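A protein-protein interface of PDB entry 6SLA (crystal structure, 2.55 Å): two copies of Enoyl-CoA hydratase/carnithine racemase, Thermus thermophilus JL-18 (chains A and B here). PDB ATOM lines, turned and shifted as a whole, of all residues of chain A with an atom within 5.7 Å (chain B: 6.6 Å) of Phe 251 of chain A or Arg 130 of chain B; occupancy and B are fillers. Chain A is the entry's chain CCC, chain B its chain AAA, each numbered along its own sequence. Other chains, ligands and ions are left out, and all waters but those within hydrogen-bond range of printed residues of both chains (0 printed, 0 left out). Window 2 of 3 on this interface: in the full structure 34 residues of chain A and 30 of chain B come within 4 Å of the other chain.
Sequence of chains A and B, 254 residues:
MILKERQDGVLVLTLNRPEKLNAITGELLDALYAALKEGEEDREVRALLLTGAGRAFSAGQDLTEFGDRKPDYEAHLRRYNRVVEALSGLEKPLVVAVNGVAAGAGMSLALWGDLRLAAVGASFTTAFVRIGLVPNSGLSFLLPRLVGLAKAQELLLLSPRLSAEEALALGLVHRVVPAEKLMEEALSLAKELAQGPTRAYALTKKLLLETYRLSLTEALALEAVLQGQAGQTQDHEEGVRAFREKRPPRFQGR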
ATOM      1  N   ARG A  46      -2.979 -23.422 -20.479  1.00  0.00           N
ATOM      2  CA  ARG A  46      -4.164 -22.609 -20.686  1.00  0.00           C
ATOM      3  C   ARG A  46      -5.395 -23.269 -20.053  1.00  0.00           C
ATOM      4  O   ARG A  46      -6.509 -22.743 -20.153  1.00  0.00           O
ATOM      5  CB  ARG A  46      -4.284 -22.258 -22.178  1.00  0.00           C
ATOM      6  CG  ARG A  46      -3.343 -21.130 -22.590  1.00  0.00           C
ATOM      7  CD  ARG A  46      -3.358 -20.772 -24.063  1.00  0.00           C
ATOM      8  NE  ARG A  46      -4.667 -20.465 -24.612  1.00  0.00           N
ATOM      9  CZ  ARG A  46      -4.960 -20.525 -25.905  1.00  0.00           C
ATOM     10  NH1 ARG A  46      -4.030 -20.884 -26.771  1.00  0.00           N
ATOM     11  NH2 ARG A  46      -6.178 -20.238 -26.333  1.00  0.00           N
ATOM     12  N   GLN A 195      -7.922 -24.062 -25.850  1.00  0.00           N
ATOM     13  CA  GLN A 195      -7.890 -23.363 -27.134  1.00  0.00           C
ATOM     14  C   GLN A 195      -8.697 -22.054 -27.051  1.00  0.00           C
ATOM     15  O   GLN A 195      -8.676 -21.244 -27.976  1.00  0.00           O
ATOM     16  CB  GLN A 195      -8.555 -24.202 -28.232  1.00  0.00           C
ATOM     17  CG  GLN A 195      -7.853 -25.493 -28.617  1.00  0.00           C
ATOM     18  CD  GLN A 195      -6.470 -25.256 -29.162  1.00  0.00           C
ATOM     19  OE1 GLN A 195      -6.251 -24.398 -30.007  1.00  0.00           O
ATOM     20  NE2 GLN A 195      -5.513 -26.003 -28.647  1.00  0.00           N
ATOM     21  N   GLY A 196      -9.462 -21.867 -25.965  1.00  0.00           N
ATOM     22  CA  GLY A 196     -10.399 -20.758 -25.869  1.00  0.00           C
ATOM     23  C   GLY A 196      -9.771 -19.511 -25.245  1.00  0.00           C
ATOM     24  O   GLY A 196      -8.574 -19.472 -24.962  1.00  0.00           O
ATOM     25  N   PRO A 197     -10.559 -18.436 -25.015  1.00  0.00           N
ATOM     26  CA  PRO A 197     -10.003 -17.149 -24.605  1.00  0.00           C
ATOM     27  C   PRO A 197      -9.638 -17.094 -23.125  1.00  0.00           C
ATOM     28  O   PRO A 197     -10.432 -16.635 -22.303  1.00  0.00           O
ATOM     29  CB  PRO A 197     -11.132 -16.169 -24.946  1.00  0.00           C
ATOM     30  CG  PRO A 197     -12.426 -16.994 -24.906  1.00  0.00           C
ATOM     31  CD  PRO A 197     -12.021 -18.418 -25.172  1.00  0.00           C
ATOM     32  N   THR A 198      -8.421 -17.541 -22.803  1.00  0.00           N
ATOM     33  CA  THR A 198      -7.982 -17.736 -21.428  1.00  0.00           C
ATOM     34  C   THR A 198      -8.224 -16.501 -20.567  1.00  0.00           C
ATOM     35  O   THR A 198      -8.676 -16.646 -19.428  1.00  0.00           O
ATOM     36  CB  THR A 198      -6.534 -18.229 -21.369  1.00  0.00           C
ATOM     37  OG1 THR A 198      -6.479 -19.310 -22.304  1.00  0.00           O
ATOM     38  CG2 THR A 198      -6.096 -18.675 -19.987  1.00  0.00           C
ATOM     39  N   ASP A 235      -7.293 -11.520 -28.154  1.00  0.00           N
ATOM     40  CA  ASP A 235      -8.382 -12.474 -28.268  1.00  0.00           C
ATOM     41  C   ASP A 235      -9.711 -11.770 -28.540  1.00  0.00           C
ATOM     42  O   ASP A 235     -10.555 -12.314 -29.253  1.00  0.00           O
ATOM     43  CB  ASP A 235      -8.432 -13.423 -27.072  1.00  0.00           C
ATOM     44  CG  ASP A 235      -7.476 -14.603 -27.185  1.00  0.00           C
ATOM     45  OD1 ASP A 235      -6.969 -14.870 -28.295  1.00  0.00           O
ATOM     46  OD2 ASP A 235      -7.262 -15.256 -26.167  1.00  0.00           O
ATOM     47  N   HIS A 236      -9.893 -10.558 -27.989  1.00  0.00           N
ATOM     48  CA  HIS A 236     -11.139  -9.849 -28.232  1.00  0.00           C
ATOM     49  C   HIS A 236     -11.193  -9.350 -29.676  1.00  0.00           C
ATOM     50  O   HIS A 236     -12.233  -9.447 -30.324  1.00  0.00           O
ATOM     51  CB  HIS A 236     -11.415  -8.759 -27.188  1.00  0.00           C
ATOM     52  CG  HIS A 236     -12.501  -7.815 -27.603  1.00  0.00           C
ATOM     53  ND1 HIS A 236     -13.845  -8.198 -27.672  1.00  0.00           N
ATOM     54  CD2 HIS A 236     -12.450  -6.530 -28.029  1.00  0.00           C
ATOM     55  CE1 HIS A 236     -14.558  -7.175 -28.108  1.00  0.00           C
ATOM     56  NE2 HIS A 236     -13.731  -6.144 -28.345  1.00  0.00           N
ATOM     57  N   GLU A 238      -9.628 -10.692 -32.176  1.00  0.00           N
ATOM     58  CA  GLU A 238      -9.877 -11.947 -32.862  1.00  0.00           C
ATOM     59  C   GLU A 238     -11.352 -12.347 -32.768  1.00  0.00           C
ATOM     60  O   GLU A 238     -11.945 -12.780 -33.754  1.00  0.00           O
ATOM     61  CB  GLU A 238      -8.940 -13.015 -32.300  1.00  0.00           C
ATOM     62  CG  GLU A 238      -9.130 -14.393 -32.911  1.00  0.00           C
ATOM     63  CD  GLU A 238      -9.150 -14.507 -34.428  1.00  0.00           C
ATOM     64  OE1 GLU A 238      -8.702 -13.568 -35.118  1.00  0.00           O
ATOM     65  OE2 GLU A 238      -9.621 -15.551 -34.921  1.00  0.00           O
ATOM     66  N   GLY A 239     -11.946 -12.188 -31.581  1.00  0.00           N
ATOM     67  CA  GLY A 239     -13.325 -12.581 -31.345  1.00  0.00           C
ATOM     68  C   GLY A 239     -14.299 -11.823 -32.247  1.00  0.00           C
ATOM     69  O   GLY A 239     -15.195 -12.424 -32.853  1.00  0.00           O
ATOM     70  N   PRO A 249     -13.359 -18.436 -34.240  1.00  0.00           N
ATOM     71  CA  PRO A 249     -12.165 -17.721 -33.784  1.00  0.00           C
ATOM     72  C   PRO A 249     -10.993 -18.660 -33.490  1.00  0.00           C
ATOM     73  O   PRO A 249     -11.204 -19.834 -33.201  1.00  0.00           O
ATOM     74  CB  PRO A 249     -12.641 -17.045 -32.494  1.00  0.00           C
ATOM     75  CG  PRO A 249     -13.739 -17.938 -31.999  1.00  0.00           C
ATOM     76  CD  PRO A 249     -14.436 -18.433 -33.240  1.00  0.00           C
ATOM     77  N   ARG A 250      -9.767 -18.129 -33.554  1.00  0.00           N
ATOM     78  CA  ARG A 250      -8.617 -18.848 -33.036  1.00  0.00           C
ATOM     79  C   ARG A 250      -7.950 -17.989 -31.972  1.00  0.00           C
ATOM     80  O   ARG A 250      -7.340 -16.969 -32.285  1.00  0.00           O
ATOM     81  CB  ARG A 250      -7.632 -19.232 -34.142  1.00  0.00           C
ATOM     82  CG  ARG A 250      -8.170 -20.298 -35.091  1.00  0.00           C
ATOM     83  CD  ARG A 250      -8.736 -21.598 -34.521  1.00  0.00           C
ATOM     84  NE  ARG A 250      -7.948 -22.087 -33.394  1.00  0.00           N
ATOM     85  CZ  ARG A 250      -7.825 -23.356 -33.021  1.00  0.00           C
ATOM     86  NH1 ARG A 250      -7.066 -23.668 -31.985  1.00  0.00           N
ATOM     87  NH2 ARG A 250      -8.447 -24.320 -33.672  1.00  0.00           N
ATOM     88  N   PHE A 251      -8.114 -18.412 -30.716  1.00  0.00           N
ATOM     89  CA  PHE A 251      -7.730 -17.621 -29.561  1.00  0.00           C
ATOM     90  C   PHE A 251      -6.338 -18.040 -29.099  1.00  0.00           C
ATOM     91  O   PHE A 251      -5.951 -19.181 -29.297  1.00  0.00           O
ATOM     92  CB  PHE A 251      -8.764 -17.827 -28.460  1.00  0.00           C
ATOM     93  CG  PHE A 251     -10.121 -17.210 -28.690  1.00  0.00           C
ATOM     94  CD1 PHE A 251     -10.256 -15.860 -28.970  1.00  0.00           C
ATOM     95  CD2 PHE A 251     -11.276 -17.974 -28.542  1.00  0.00           C
ATOM     96  CE1 PHE A 251     -11.514 -15.294 -29.133  1.00  0.00           C
ATOM     97  CE2 PHE A 251     -12.531 -17.401 -28.697  1.00  0.00           C
ATOM     98  CZ  PHE A 251     -12.653 -16.060 -28.997  1.00  0.00           C
ATOM     99  N   GLN A 252      -5.608 -17.121 -28.463  1.00  0.00           N
ATOM    100  CA  GLN A 252      -4.255 -17.411 -28.003  1.00  0.00           C
ATOM    101  C   GLN A 252      -4.159 -17.275 -26.481  1.00  0.00           C
ATOM    102  O   GLN A 252      -3.205 -17.761 -25.866  1.00  0.00           O
ATOM    103  CB  GLN A 252      -3.232 -16.484 -28.663  1.00  0.00           C
ATOM    104  CG  GLN A 252      -3.505 -16.122 -30.113  1.00  0.00           C
ATOM    105  CD  GLN A 252      -2.580 -15.014 -30.582  1.00  0.00           C
ATOM    106  OE1 GLN A 252      -1.591 -15.260 -31.275  1.00  0.00           O
ATOM    107  NE2 GLN A 252      -2.900 -13.772 -30.232  1.00  0.00           N
ATOM    108  N   GLY A 253      -5.140 -16.587 -25.877  1.00  0.00           N
ATOM    109  CA  GLY A 253      -5.148 -16.351 -24.439  1.00  0.00           C
ATOM    110  C   GLY A 253      -4.381 -15.095 -24.030  1.00  0.00           C
ATOM    111  O   GLY A 253      -3.785 -15.101 -22.952  1.00  0.00           O
ATOM    112  N   THR B 125     -28.432 -16.931 -25.111  1.00  0.00           N
ATOM    113  CA  THR B 125     -27.014 -17.271 -25.114  1.00  0.00           C
ATOM    114  C   THR B 125     -26.220 -16.106 -24.518  1.00  0.00           C
ATOM    115  O   THR B 125     -26.428 -14.954 -24.860  1.00  0.00           O
ATOM    116  CB  THR B 125     -26.545 -17.764 -26.490  1.00  0.00           C
ATOM    117  OG1 THR B 125     -25.131 -17.943 -26.381  1.00  0.00           O
ATOM    118  CG2 THR B 125     -26.840 -16.794 -27.627  1.00  0.00           C
ATOM    119  N   ALA B 127     -22.996 -15.463 -24.839  1.00  0.00           N
ATOM    120  CA  ALA B 127     -22.318 -14.930 -26.016  1.00  0.00           C
ATOM    121  C   ALA B 127     -20.964 -14.315 -25.651  1.00  0.00           C
ATOM    122  O   ALA B 127     -20.023 -14.481 -26.406  1.00  0.00           O
ATOM    123  CB  ALA B 127     -23.187 -13.938 -26.767  1.00  0.00           C
ATOM    124  N   PHE B 128     -20.896 -13.549 -24.557  1.00  0.00           N
ATOM    125  CA  PHE B 128     -19.707 -12.774 -24.237  1.00  0.00           C
ATOM    126  C   PHE B 128     -18.371 -13.468 -24.534  1.00  0.00           C
ATOM    127  O   PHE B 128     -17.518 -12.874 -25.178  1.00  0.00           O
ATOM    128  CB  PHE B 128     -19.738 -12.303 -22.792  1.00  0.00           C
ATOM    129  CG  PHE B 128     -20.881 -11.367 -22.505  1.00  0.00           C
ATOM    130  CD1 PHE B 128     -20.824 -10.046 -22.912  1.00  0.00           C
ATOM    131  CD2 PHE B 128     -22.016 -11.804 -21.840  1.00  0.00           C
ATOM    132  CE1 PHE B 128     -21.864  -9.173 -22.623  1.00  0.00           C
ATOM    133  CE2 PHE B 128     -23.055 -10.935 -21.568  1.00  0.00           C
ATOM    134  CZ  PHE B 128     -22.978  -9.620 -21.959  1.00  0.00           C
ATOM    135  N   VAL B 129     -18.162 -14.685 -24.049  1.00  0.00           N
ATOM    136  CA  VAL B 129     -16.852 -15.323 -24.100  1.00  0.00           C
ATOM    137  C   VAL B 129     -16.443 -15.648 -25.546  1.00  0.00           C
ATOM    138  O   VAL B 129     -15.254 -15.724 -25.856  1.00  0.00           O
ATOM    139  CB  VAL B 129     -16.760 -16.575 -23.195  1.00  0.00           C
ATOM    140  CG1 VAL B 129     -16.595 -16.201 -21.732  1.00  0.00           C
ATOM    141  CG2 VAL B 129     -17.846 -17.601 -23.422  1.00  0.00           C
ATOM    142  N   ARG B 130     -17.447 -15.842 -26.418  1.00  0.00           N
ATOM    143  CA  ARG B 130     -17.219 -16.160 -27.819  1.00  0.00           C
ATOM    144  C   ARG B 130     -16.537 -14.995 -28.531  1.00  0.00           C
ATOM    145  O   ARG B 130     -15.947 -15.183 -29.579  1.00  0.00           O
ATOM    146  CB  ARG B 130     -18.531 -16.517 -28.526  1.00  0.00           C
ATOM    147  CG  ARG B 130     -19.067 -17.892 -28.139  1.00  0.00           C
ATOM    148  CD  ARG B 130     -20.361 -18.294 -28.798  1.00  0.00           C
ATOM    149  NE  ARG B 130     -20.451 -19.705 -29.163  1.00  0.00           N
ATOM    150  CZ  ARG B 130     -20.293 -20.742 -28.348  1.00  0.00           C
ATOM    151  NH1 ARG B 130     -19.987 -20.557 -27.082  1.00  0.00           N
ATOM    152  NH2 ARG B 130     -20.414 -21.979 -28.791  1.00  0.00           N
ATOM    153  N   ILE B 131     -16.631 -13.792 -27.969  1.00  0.00           N
ATOM    154  CA  ILE B 131     -16.061 -12.564 -28.520  1.00  0.00           C
ATOM    155  C   ILE B 131     -14.836 -12.173 -27.674  1.00  0.00           C
ATOM    156  O   ILE B 131     -14.333 -11.066 -27.785  1.00  0.00           O
ATOM    157  CB  ILE B 131     -17.121 -11.435 -28.444  1.00  0.00           C
ATOM    158  CG1 ILE B 131     -18.480 -11.737 -29.091  1.00  0.00           C
ATOM    159  CG2 ILE B 131     -16.552 -10.109 -28.887  1.00  0.00           C
ATOM    160  CD1 ILE B 131     -18.436 -12.120 -30.550  1.00  0.00           C
ATOM    161  N   GLY B 132     -14.402 -13.074 -26.786  1.00  0.00           N
ATOM    162  CA  GLY B 132     -13.311 -12.830 -25.853  1.00  0.00           C
ATOM    163  C   GLY B 132     -13.597 -11.773 -24.783  1.00  0.00           C
ATOM    164  O   GLY B 132     -12.662 -11.139 -24.292  1.00  0.00           O
ATOM    165  N   LEU B 133     -14.879 -11.614 -24.400  1.00  0.00           N
ATOM    166  CA  LEU B 133     -15.308 -10.625 -23.419  1.00  0.00           C
ATOM    167  C   LEU B 133     -15.844 -11.294 -22.159  1.00  0.00           C
ATOM    168  O   LEU B 133     -16.141 -12.481 -22.144  1.00  0.00           O
ATOM    169  CB  LEU B 133     -16.361  -9.718 -24.055  1.00  0.00           C
ATOM    170  CG  LEU B 133     -15.838  -8.705 -25.073  1.00  0.00           C
ATOM    171  CD1 LEU B 133     -16.950  -7.869 -25.667  1.00  0.00           C
ATOM    172  CD2 LEU B 133     -14.770  -7.792 -24.470  1.00  0.00           C
ATOM    173  N   LEU B 156     -21.993 -19.255 -18.753  1.00  0.00           N
ATOM    174  CA  LEU B 156     -21.057 -18.187 -19.090  1.00  0.00           C
ATOM    175  C   LEU B 156     -19.815 -18.715 -19.819  1.00  0.00           C
ATOM    176  O   LEU B 156     -19.398 -18.126 -20.824  1.00  0.00           O
ATOM    177  CB  LEU B 156     -20.680 -17.412 -17.825  1.00  0.00           C
ATOM    178  CG  LEU B 156     -21.793 -16.521 -17.298  1.00  0.00           C
ATOM    179  CD1 LEU B 156     -21.412 -15.933 -15.935  1.00  0.00           C
ATOM    180  CD2 LEU B 156     -22.093 -15.412 -18.283  1.00  0.00           C
ATOM    181  N   LEU B 157     -19.237 -19.820 -19.333  1.00  0.00           N
ATOM    182  CA  LEU B 157     -17.923 -20.205 -19.858  1.00  0.00           C
ATOM    183  C   LEU B 157     -18.070 -20.959 -21.179  1.00  0.00           C
ATOM    184  O   LEU B 157     -17.169 -20.877 -22.003  1.00  0.00           O
ATOM    185  CB  LEU B 157     -17.116 -21.004 -18.829  1.00  0.00           C
ATOM    186  CG  LEU B 157     -16.782 -20.282 -17.526  1.00  0.00           C
ATOM    187  CD1 LEU B 157     -16.229 -21.243 -16.487  1.00  0.00           C
ATOM    188  CD2 LEU B 157     -15.791 -19.164 -17.788  1.00  0.00           C
ATOM    189  N   LEU B 158     -19.196 -21.661 -21.393  1.00  0.00           N
ATOM    190  CA  LEU B 158     -19.357 -22.483 -22.589  1.00  0.00           C
ATOM    191  C   LEU B 158     -20.302 -21.810 -23.583  1.00  0.00           C
ATOM    192  O   LEU B 158     -20.341 -22.181 -24.749  1.00  0.00           O
ATOM    193  CB  LEU B 158     -19.875 -23.879 -22.212  1.00  0.00           C
ATOM    194  CG  LEU B 158     -18.951 -24.713 -21.331  1.00  0.00           C
ATOM    195  CD1 LEU B 158     -19.493 -26.133 -21.201  1.00  0.00           C
ATOM    196  CD2 LEU B 158     -17.514 -24.691 -21.882  1.00  0.00           C
ATOM    197  N   SER B 159     -21.078 -20.834 -23.096  1.00  0.00           N
ATOM    198  CA  SER B 159     -22.026 -20.101 -23.923  1.00  0.00           C
ATOM    199  C   SER B 159     -22.900 -21.027 -24.773  1.00  0.00           C
ATOM    200  O   SER B 159     -23.043 -20.822 -25.971  1.00  0.00           O
ATOM    201  CB  SER B 159     -21.310 -19.083 -24.767  1.00  0.00           C
ATOM    202  OG  SER B 159     -22.245 -18.303 -25.504  1.00  0.00           O
ATOM    203  N   PRO B 160     -23.572 -22.050 -24.220  1.00  0.00           N
ATOM    204  CA  PRO B 160     -24.567 -22.793 -25.011  1.00  0.00           C
ATOM    205  C   PRO B 160     -25.789 -21.912 -25.344  1.00  0.00           C
ATOM    206  O   PRO B 160     -26.041 -20.872 -24.730  1.00  0.00           O
ATOM    207  CB  PRO B 160     -24.973 -23.934 -24.043  1.00  0.00           C
ATOM    208  CG  PRO B 160     -24.764 -23.323 -22.650  1.00  0.00           C
ATOM    209  CD  PRO B 160     -23.507 -22.488 -22.816  1.00  0.00           C
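No position is printed for both chains. Of the 6 pairs that touch across the chains among the printed residues, none has its exchanged pair printed and touching as well.
Phe 251 of chain A touches just one residue of chain B: Arg 130. Phe 128 of chain B touches none of the printed residues of chain A. Printed residues of chain A within 4 Å of Val 129 of chain B: Pro 197. Arg 130 of chain B touches just one residue of chain A: Phe 251. Printed residues of chain A within 4 Å of Ile 131 of chain B: His 236 (2.9 Å) and Gly 239 (3.9 Å). The nearest printed residue of chain B that does not touch Phe 251 of chain A is Val 129 of chain B (4.1 Å). The nearest residue of chain A that does not touch Arg 130 of chain B is Gly 239 of chain A (4.1 Å).
Hydrophobic or aromatic side chains of chain B that line the printed part of chain A: Ile 131 and Leu 133. Of the 14 printed residues of chain A, 4 touch a printed residue of chain B. Along chain A the printed residues that touch a printed residue of chain B span positions 197 to 251. Among the printed residues, no Asp or Glu carboxylate lies within 4 Å of a Lys or Arg side-chain nitrogen of the other chain.
O of Phe 128 of chain B sits at hydrogen-bond distance from N of Leu 133 of chain B (3.0 Å). NH2 of Arg 46 of chain A sits at hydrogen-bond distance from O of Phe 251 of chain A (3.2 Å). The guanidinium group (NH1) of Arg 130 of chain B lies close to the backbone carbonyl oxygen (O) of Ser 159 of chain B, at 3.3 Å. The backbone carbonyl oxygen of Leu 158 of chain B is in hydrogen-bond range of the guanidinium group of Arg 130 of chain B (2.9 Å).
Among the printed residues, pairs that only touch across the chains: Pro 197 of chain A with Val 129 of chain B, His 236 of chain A with Leu 133 of chain B, Phe 251 of chain A with Arg 130 of chain B, Gly 239 of chain A with Ile 131 of chain B and His 236 of chain A with Gly 132 of chain B.
O of Ile 131 of chain B is in hydrogen-bond range of ND1 of His 236 of chain A, 2.9 Å away.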
